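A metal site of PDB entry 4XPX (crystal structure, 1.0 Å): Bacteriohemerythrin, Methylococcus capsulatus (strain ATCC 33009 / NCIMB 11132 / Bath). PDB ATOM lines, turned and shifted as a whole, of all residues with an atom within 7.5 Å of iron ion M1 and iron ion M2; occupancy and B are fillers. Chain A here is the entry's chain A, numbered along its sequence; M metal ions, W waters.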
ATOM      1  N   THR A  12     -21.438  30.166  32.662  1.00  0.00           N
ATOM      2  CA  THR A  12     -20.566  29.286  33.411  1.00  0.00           C
ATOM      3  C   THR A  12     -20.485  29.615  34.856  1.00  0.00           C
ATOM      4  O   THR A  12     -19.891  28.826  35.627  1.00  0.00           O
ATOM      5  CB  THR A  12     -19.145  29.281  32.859  1.00  0.00           C
ATOM      6  OG1 THR A  12     -18.558  30.567  33.070  1.00  0.00           O
ATOM      7  CG2 THR A  12     -19.077  28.841  31.404  1.00  0.00           C
ATOM      8  N   ALA A  17     -14.590  33.894  31.920  1.00  0.00           N
ATOM      9  CA  ALA A  17     -14.896  32.977  30.877  1.00  0.00           C
ATOM     10  C   ALA A  17     -16.092  33.399  30.114  1.00  0.00           C
ATOM     11  O   ALA A  17     -16.130  33.352  28.864  1.00  0.00           O
ATOM     12  CB  ALA A  17     -15.106  31.581  31.449  1.00  0.00           C
ATOM     13  N   ASP A  18     -17.137  33.832  30.789  1.00  0.00           N
ATOM     14  CA  ASP A  18     -18.302  34.355  30.108  1.00  0.00           C
ATOM     15  C   ASP A  18     -17.933  35.529  29.205  1.00  0.00           C
ATOM     16  O   ASP A  18     -18.425  35.628  28.069  1.00  0.00           O
ATOM     17  CB  ASP A  18     -19.367  34.798  31.086  1.00  0.00           C
ATOM     18  CG  ASP A  18     -20.016  33.623  31.846  1.00  0.00           C
ATOM     19  OD1 ASP A  18     -19.984  32.483  31.464  1.00  0.00           O
ATOM     20  OD2 ASP A  18     -20.658  34.020  32.897  1.00  0.00           O
ATOM     21  N   GLN A  20     -14.983  36.237  27.818  1.00  0.00           N
ATOM     22  CA  GLN A  20     -14.221  35.764  26.653  1.00  0.00           C
ATOM     23  C   GLN A  20     -15.120  35.033  25.687  1.00  0.00           C
ATOM     24  O   GLN A  20     -14.958  35.178  24.455  1.00  0.00           O
ATOM     25  CB  GLN A  20     -13.020  34.859  27.118  1.00  0.00           C
ATOM     26  CG  GLN A  20     -11.978  35.666  27.872  1.00  0.00           C
ATOM     27  CD  GLN A  20     -10.820  34.815  28.339  1.00  0.00           C
ATOM     28  OE1 GLN A  20     -10.896  33.641  28.539  1.00  0.00           O
ATOM     29  NE2 GLN A  20      -9.648  35.442  28.400  1.00  0.00           N
ATOM     30  N   HIS A  21     -16.086  34.259  26.194  1.00  0.00           N
ATOM     31  CA  HIS A  21     -17.045  33.605  25.264  1.00  0.00           C
ATOM     32  C   HIS A  21     -17.814  34.618  24.469  1.00  0.00           C
ATOM     33  O   HIS A  21     -18.045  34.463  23.260  1.00  0.00           O
ATOM     34  CB  HIS A  21     -17.994  32.702  26.037  1.00  0.00           C
ATOM     35  CG  HIS A  21     -17.304  31.510  26.627  1.00  0.00           C
ATOM     36  ND1 HIS A  21     -17.796  30.820  27.721  1.00  0.00           N
ATOM     37  CD2 HIS A  21     -16.152  30.855  26.272  1.00  0.00           C
ATOM     38  CE1 HIS A  21     -16.976  29.787  27.954  1.00  0.00           C
ATOM     39  NE2 HIS A  21     -15.947  29.773  27.119  1.00  0.00           N
ATOM     40  N   ILE A  24     -15.654  35.826  21.708  1.00  0.00           N
ATOM     41  CA  ILE A  24     -15.571  34.824  20.669  1.00  0.00           C
ATOM     42  C   ILE A  24     -16.810  34.874  19.783  1.00  0.00           C
ATOM     43  O   ILE A  24     -16.709  34.810  18.545  1.00  0.00           O
ATOM     44  CB  ILE A  24     -15.312  33.450  21.269  1.00  0.00           C
ATOM     45  CG1 ILE A  24     -13.925  33.352  21.867  1.00  0.00           C
ATOM     46  CG2 ILE A  24     -15.518  32.369  20.232  1.00  0.00           C
ATOM     47  CD1 ILE A  24     -13.680  32.174  22.777  1.00  0.00           C
ATOM     48  N   VAL A  54      -9.226  32.798  20.413  1.00  0.00           N
ATOM     49  CA  VAL A  54      -9.648  31.511  20.912  1.00  0.00           C
ATOM     50  C   VAL A  54      -8.482  30.817  21.643  1.00  0.00           C
ATOM     51  O   VAL A  54      -8.658  30.263  22.767  1.00  0.00           O
ATOM     52  CB  VAL A  54     -10.210  30.645  19.820  1.00  0.00           C
ATOM     53  CG1 VAL A  54     -10.428  29.189  20.285  1.00  0.00           C
ATOM     54  CG2 VAL A  54     -11.553  31.227  19.346  1.00  0.00           C
ATOM     55  N   HIS A  57      -8.054  32.386  24.964  1.00  0.00           N
ATOM     56  CA  HIS A  57      -9.126  31.984  25.839  1.00  0.00           C
ATOM     57  C   HIS A  57      -8.831  30.587  26.420  1.00  0.00           C
ATOM     58  O   HIS A  57      -9.017  30.335  27.651  1.00  0.00           O
ATOM     59  CB  HIS A  57     -10.433  31.975  25.064  1.00  0.00           C
ATOM     60  CG  HIS A  57     -11.553  31.277  25.801  1.00  0.00           C
ATOM     61  ND1 HIS A  57     -11.991  31.657  27.045  1.00  0.00           N
ATOM     62  CD2 HIS A  57     -12.264  30.170  25.489  1.00  0.00           C
ATOM     63  CE1 HIS A  57     -12.943  30.795  27.443  1.00  0.00           C
ATOM     64  NE2 HIS A  57     -13.124  29.868  26.523  1.00  0.00           N
ATOM     65  N   PHE A  58      -8.441  29.656  25.577  1.00  0.00           N
ATOM     66  CA  PHE A  58      -8.128  28.313  26.057  1.00  0.00           C
ATOM     67  C   PHE A  58      -7.038  28.364  27.072  1.00  0.00           C
ATOM     68  O   PHE A  58      -7.109  27.651  28.117  1.00  0.00           O
ATOM     69  CB  PHE A  58      -7.740  27.401  24.888  1.00  0.00           C
ATOM     70  CG  PHE A  58      -8.903  27.065  23.940  1.00  0.00           C
ATOM     71  CD1 PHE A  58      -8.568  26.427  22.744  1.00  0.00           C
ATOM     72  CD2 PHE A  58     -10.221  27.299  24.240  1.00  0.00           C
ATOM     73  CE1 PHE A  58      -9.566  26.042  21.865  1.00  0.00           C
ATOM     74  CE2 PHE A  58     -11.168  26.895  23.326  1.00  0.00           C
ATOM     75  CZ  PHE A  58     -10.869  26.257  22.172  1.00  0.00           C
ATOM     76  N   GLU A  61      -8.503  29.588  30.439  1.00  0.00           N
ATOM     77  CA  GLU A  61      -9.233  28.551  31.142  1.00  0.00           C
ATOM     78  C   GLU A  61      -8.230  27.510  31.685  1.00  0.00           C
ATOM     79  O   GLU A  61      -8.403  27.044  32.859  1.00  0.00           O
ATOM     80  CB  GLU A  61     -10.192  27.794  30.215  1.00  0.00           C
ATOM     81  CG  GLU A  61     -11.443  28.583  29.831  1.00  0.00           C
ATOM     82  CD  GLU A  61     -12.427  27.712  29.062  1.00  0.00           C
ATOM     83  OE1 GLU A  61     -12.080  26.605  28.712  1.00  0.00           O
ATOM     84  OE2 GLU A  61     -13.577  28.237  28.851  1.00  0.00           O
ATOM     85  N   GLU A  62      -7.273  27.107  30.919  1.00  0.00           N
ATOM     86  CA  GLU A  62      -6.361  26.029  31.345  1.00  0.00           C
ATOM     87  C   GLU A  62      -5.544  26.468  32.516  1.00  0.00           C
ATOM     88  O   GLU A  62      -5.314  25.643  33.452  1.00  0.00           O
ATOM     89  CB  GLU A  62      -5.465  25.616  30.176  1.00  0.00           C
ATOM     90  CG  GLU A  62      -6.231  24.861  29.121  1.00  0.00           C
ATOM     91  CD  GLU A  62      -5.549  24.786  27.776  1.00  0.00           C
ATOM     92  OE1 GLU A  62      -4.262  24.907  27.724  1.00  0.00           O
ATOM     93  OE2 GLU A  62      -6.203  24.521  26.729  1.00  0.00           O
ATOM     94  N   MET A  65      -7.900  26.334  35.574  1.00  0.00           N
ATOM     95  CA  MET A  65      -8.199  24.966  35.916  1.00  0.00           C
ATOM     96  C   MET A  65      -7.018  24.273  36.565  1.00  0.00           C
ATOM     97  O   MET A  65      -7.177  23.558  37.612  1.00  0.00           O
ATOM     98  CB  MET A  65      -8.625  24.153  34.690  1.00  0.00           C
ATOM     99  CG  MET A  65     -10.043  24.464  34.206  1.00  0.00           C
ATOM    100  SD  MET A  65     -10.582  23.356  32.848  1.00  0.00           S
ATOM    101  CE  MET A  65      -9.664  24.033  31.418  1.00  0.00           C
ATOM    102  N   HIS A  76     -10.288  18.268  29.540  1.00  0.00           N
ATOM    103  CA  HIS A  76     -10.757  19.522  28.969  1.00  0.00           C
ATOM    104  C   HIS A  76      -9.711  20.116  28.082  1.00  0.00           C
ATOM    105  O   HIS A  76      -9.995  20.534  26.908  1.00  0.00           O
ATOM    106  CB  HIS A  76     -11.131  20.438  30.122  1.00  0.00           C
ATOM    107  CG  HIS A  76     -11.842  21.672  29.717  1.00  0.00           C
ATOM    108  ND1 HIS A  76     -12.819  22.182  30.530  1.00  0.00           N
ATOM    109  CD2 HIS A  76     -11.710  22.549  28.677  1.00  0.00           C
ATOM    110  CE1 HIS A  76     -13.263  23.311  29.924  1.00  0.00           C
ATOM    111  NE2 HIS A  76     -12.610  23.577  28.830  1.00  0.00           N
ATOM    112  N   LYS A  77      -8.457  20.163  28.515  1.00  0.00           N
ATOM    113  CA  LYS A  77      -7.367  20.645  27.654  1.00  0.00           C
ATOM    114  C   LYS A  77      -7.273  19.843  26.400  1.00  0.00           C
ATOM    115  O   LYS A  77      -6.967  20.403  25.318  1.00  0.00           O
ATOM    116  CB  LYS A  77      -6.066  20.627  28.416  1.00  0.00           C
ATOM    117  CG  LYS A  77      -4.896  21.133  27.581  1.00  0.00           C
ATOM    118  CD  LYS A  77      -3.652  21.305  28.380  1.00  0.00           C
ATOM    119  CE  LYS A  77      -2.517  21.972  27.606  1.00  0.00           C
ATOM    120  NZ  LYS A  77      -2.105  21.179  26.482  1.00  0.00           N
ATOM    121  N   GLU A  79      -9.657  18.503  24.681  1.00  0.00           N
ATOM    122  CA  GLU A  79     -10.674  19.027  23.755  1.00  0.00           C
ATOM    123  C   GLU A  79     -10.210  20.302  23.091  1.00  0.00           C
ATOM    124  O   GLU A  79     -10.339  20.497  21.877  1.00  0.00           O
ATOM    125  CB  GLU A  79     -12.013  19.238  24.427  1.00  0.00           C
ATOM    126  CG  GLU A  79     -12.611  18.032  25.132  1.00  0.00           C
ATOM    127  CD  GLU A  79     -12.830  16.779  24.326  1.00  0.00           C
ATOM    128  OE1 GLU A  79     -12.863  16.852  23.082  1.00  0.00           O
ATOM    129  OE2 GLU A  79     -12.942  15.626  24.956  1.00  0.00           O
ATOM    130  N   HIS A  80      -9.679  21.213  23.887  1.00  0.00           N
ATOM    131  CA  HIS A  80      -9.108  22.480  23.331  1.00  0.00           C
ATOM    132  C   HIS A  80      -8.060  22.172  22.314  1.00  0.00           C
ATOM    133  O   HIS A  80      -8.047  22.775  21.196  1.00  0.00           O
ATOM    134  CB  HIS A  80      -8.468  23.303  24.424  1.00  0.00           C
ATOM    135  CG  HIS A  80      -9.416  23.895  25.408  1.00  0.00           C
ATOM    136  ND1 HIS A  80      -8.940  24.561  26.512  1.00  0.00           N
ATOM    137  CD2 HIS A  80     -10.762  24.022  25.470  1.00  0.00           C
ATOM    138  CE1 HIS A  80      -9.993  25.039  27.192  1.00  0.00           C
ATOM    139  NE2 HIS A  80     -11.118  24.742  26.550  1.00  0.00           N
ATOM    140  N   TRP A 112     -18.966  23.674  17.402  1.00  0.00           N
ATOM    141  CA  TRP A 112     -18.010  23.266  18.425  1.00  0.00           C
ATOM    142  C   TRP A 112     -18.292  24.045  19.704  1.00  0.00           C
ATOM    143  O   TRP A 112     -18.315  23.433  20.822  1.00  0.00           O
ATOM    144  CB  TRP A 112     -16.582  23.507  17.925  1.00  0.00           C
ATOM    145  CG  TRP A 112     -15.540  22.951  18.834  1.00  0.00           C
ATOM    146  CD1 TRP A 112     -14.949  21.710  18.715  1.00  0.00           C
ATOM    147  CD2 TRP A 112     -15.016  23.535  20.016  1.00  0.00           C
ATOM    148  NE1 TRP A 112     -14.079  21.515  19.716  1.00  0.00           N
ATOM    149  CE2 TRP A 112     -14.091  22.616  20.554  1.00  0.00           C
ATOM    150  CE3 TRP A 112     -15.169  24.732  20.652  1.00  0.00           C
ATOM    151  CZ2 TRP A 112     -13.372  22.847  21.713  1.00  0.00           C
ATOM    152  CZ3 TRP A 112     -14.477  25.008  21.801  1.00  0.00           C
ATOM    153  CH2 TRP A 112     -13.570  24.032  22.326  1.00  0.00           C
ATOM    154  N   LEU A 113     -18.495  25.348  19.612  1.00  0.00           N
ATOM    155  CA  LEU A 113     -18.691  26.198  20.791  1.00  0.00           C
ATOM    156  C   LEU A 113     -20.002  25.858  21.490  1.00  0.00           C
ATOM    157  O   LEU A 113     -20.012  25.830  22.756  1.00  0.00           O
ATOM    158  CB  LEU A 113     -18.721  27.663  20.387  1.00  0.00           C
ATOM    159  CG  LEU A 113     -17.339  28.240  19.918  1.00  0.00           C
ATOM    160  CD1 LEU A 113     -17.587  29.562  19.182  1.00  0.00           C
ATOM    161  CD2 LEU A 113     -16.443  28.452  21.145  1.00  0.00           C
ATOM    162  N   HIS A 116     -19.301  22.670  23.310  1.00  0.00           N
ATOM    163  CA  HIS A 116     -18.264  22.685  24.330  1.00  0.00           C
ATOM    164  C   HIS A 116     -18.646  23.534  25.535  1.00  0.00           C
ATOM    165  O   HIS A 116     -18.356  23.153  26.677  1.00  0.00           O
ATOM    166  CB  HIS A 116     -16.986  23.334  23.714  1.00  0.00           C
ATOM    167  CG  HIS A 116     -15.803  23.356  24.644  1.00  0.00           C
ATOM    168  ND1 HIS A 116     -14.964  22.275  24.827  1.00  0.00           N
ATOM    169  CD2 HIS A 116     -15.351  24.346  25.435  1.00  0.00           C
ATOM    170  CE1 HIS A 116     -14.011  22.649  25.683  1.00  0.00           C
ATOM    171  NE2 HIS A 116     -14.188  23.895  26.084  1.00  0.00           N
ATOM    172  N   ILE A 117     -19.233  24.705  25.322  1.00  0.00           N
ATOM    173  CA  ILE A 117     -19.475  25.578  26.450  1.00  0.00           C
ATOM    174  C   ILE A 117     -20.439  24.940  27.461  1.00  0.00           C
ATOM    175  O   ILE A 117     -20.146  24.866  28.644  1.00  0.00           O
ATOM    176  CB  ILE A 117     -19.837  26.998  26.025  1.00  0.00           C
ATOM    177  CG1 ILE A 117     -18.659  27.645  25.319  1.00  0.00           C
ATOM    178  CG2 ILE A 117     -20.284  27.803  27.260  1.00  0.00           C
ATOM    179  CD1 ILE A 117     -19.024  28.899  24.549  1.00  0.00           C
ATOM    180  N   VAL A 120     -18.814  21.139  28.570  1.00  0.00           N
ATOM    181  CA  VAL A 120     -17.443  21.026  29.042  1.00  0.00           C
ATOM    182  C   VAL A 120     -17.127  22.227  29.934  1.00  0.00           C
ATOM    183  O   VAL A 120     -16.748  22.053  31.093  1.00  0.00           O
ATOM    184  CB  VAL A 120     -16.415  20.892  27.862  1.00  0.00           C
ATOM    185  CG1 VAL A 120     -15.028  20.598  28.421  1.00  0.00           C
ATOM    186  CG2 VAL A 120     -16.860  19.797  26.906  1.00  0.00           C
ATOM    187  N   ASP A 121     -17.294  23.463  29.461  1.00  0.00           N
ATOM    188  CA  ASP A 121     -16.972  24.607  30.278  1.00  0.00           C
ATOM    189  C   ASP A 121     -17.865  24.742  31.483  1.00  0.00           C
ATOM    190  O   ASP A 121     -17.384  25.104  32.581  1.00  0.00           O
ATOM    191  CB  ASP A 121     -16.997  25.931  29.475  1.00  0.00           C
ATOM    192  CG  ASP A 121     -15.855  26.091  28.500  1.00  0.00           C
ATOM    193  OD1 ASP A 121     -14.867  25.334  28.590  1.00  0.00           O
ATOM    194  OD2 ASP A 121     -16.002  27.006  27.641  1.00  0.00           O
ATOM    195  N   LYS A 122     -19.164  24.531  31.375  1.00  0.00           N
ATOM    196  CA  LYS A 122     -20.001  24.719  32.534  1.00  0.00           C
ATOM    197  C   LYS A 122     -19.524  23.881  33.683  1.00  0.00           C
ATOM    198  O   LYS A 122     -19.790  24.213  34.893  1.00  0.00           O
ATOM    199  CB  LYS A 122     -21.481  24.447  32.238  1.00  0.00           C
ATOM    200  CG  LYS A 122     -22.165  25.582  31.525  1.00  0.00           C
ATOM    201  CD  LYS A 122     -23.689  25.233  31.368  1.00  0.00           C
ATOM    202  CE  LYS A 122     -24.393  26.298  30.547  1.00  0.00           C
ATOM    203  NZ  LYS A 122     -25.872  26.117  30.756  1.00  0.00           N
ATOM    204  N   TYR A 124     -16.686  23.425  34.948  1.00  0.00           N
ATOM    205  CA  TYR A 124     -15.715  24.017  35.836  1.00  0.00           C
ATOM    206  C   TYR A 124     -16.265  25.106  36.735  1.00  0.00           C
ATOM    207  O   TYR A 124     -15.542  25.669  37.524  1.00  0.00           O
ATOM    208  CB  TYR A 124     -14.418  24.523  35.103  1.00  0.00           C
ATOM    209  CG  TYR A 124     -14.618  25.581  34.039  1.00  0.00           C
ATOM    210  CD1 TYR A 124     -15.339  26.739  34.259  1.00  0.00           C
ATOM    211  CD2 TYR A 124     -13.989  25.439  32.793  1.00  0.00           C
ATOM    212  CE1 TYR A 124     -15.481  27.714  33.269  1.00  0.00           C
ATOM    213  CE2 TYR A 124     -14.152  26.361  31.808  1.00  0.00           C
ATOM    214  CZ  TYR A 124     -14.895  27.488  32.007  1.00  0.00           C
ATOM    215  OH  TYR A 124     -15.131  28.447  31.053  1.00  0.00           O
HETATM  216 FE    FE M   1     -14.517  28.270  26.837  1.00  0.00          FE
HETATM  217 FE    FE M   2     -13.082  25.183  27.416  1.00  0.00          FE
HETATM  218  O   HOH W   1     -15.162  28.147  24.403  1.00  0.00           O
HETATM  219  O   HOH W   2     -13.467  26.861  25.926  1.00  0.00           O
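The side-chain carboxylate (OE2) of Glu 61 sits close to the side-chain hydroxyl (OH) of Tyr 124 (2.7 Å). The side-chain amide oxygen (OE1) of Gln 20 lies within hydrogen-bond range of a ring nitrogen (ND1) of His 57 (2.7 Å). A ring nitrogen (ND1) of His 76 sits at hydrogen-bond distance from the side-chain sulfur (SD) of Met 65, 3.4 Å away. ND1 of His 80 lies within hydrogen-bond range of OE2 of Glu 62, 2.7 Å away. ND1 of His 21 sits close to O of Ala 17 (3.2 Å).
The nearest printed residue that does not touch iron ion M1 is His 116 (4.2 Å).
Within 4 Å of iron ion M2: Glu 61, His 76, His 80, His 116 and Asp 121. Along chain A the residues within 4 Å of iron ion M2 span positions 61 to 121. The nearest printed residue that does not touch iron ion M2 is Tyr 124 (4.7 Å).
Iron ion M1 is bound by water W2 (2.0 Å), a ring nitrogen (NE2) of His 21 (2.1 Å), the side-chain carboxylate of Asp 121 (2.1 Å), a ring nitrogen (NE2) of His 57 (2.1 Å), the side-chain carboxylate of Glu 61 (2.2 Å) and water W1 (2.5 Å). Iron ion M1 has six donor atoms within binding distance.
Iron ion M2 is bound by OD1 of Asp 121 (2.1 Å), NE2 of His 116 (2.2 Å), OE1 of Glu 61 (2.2 Å), NE2 of His 80 (2.2 Å), NE2 of His 76 (2.2 Å) and water W2 (2.3 Å).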
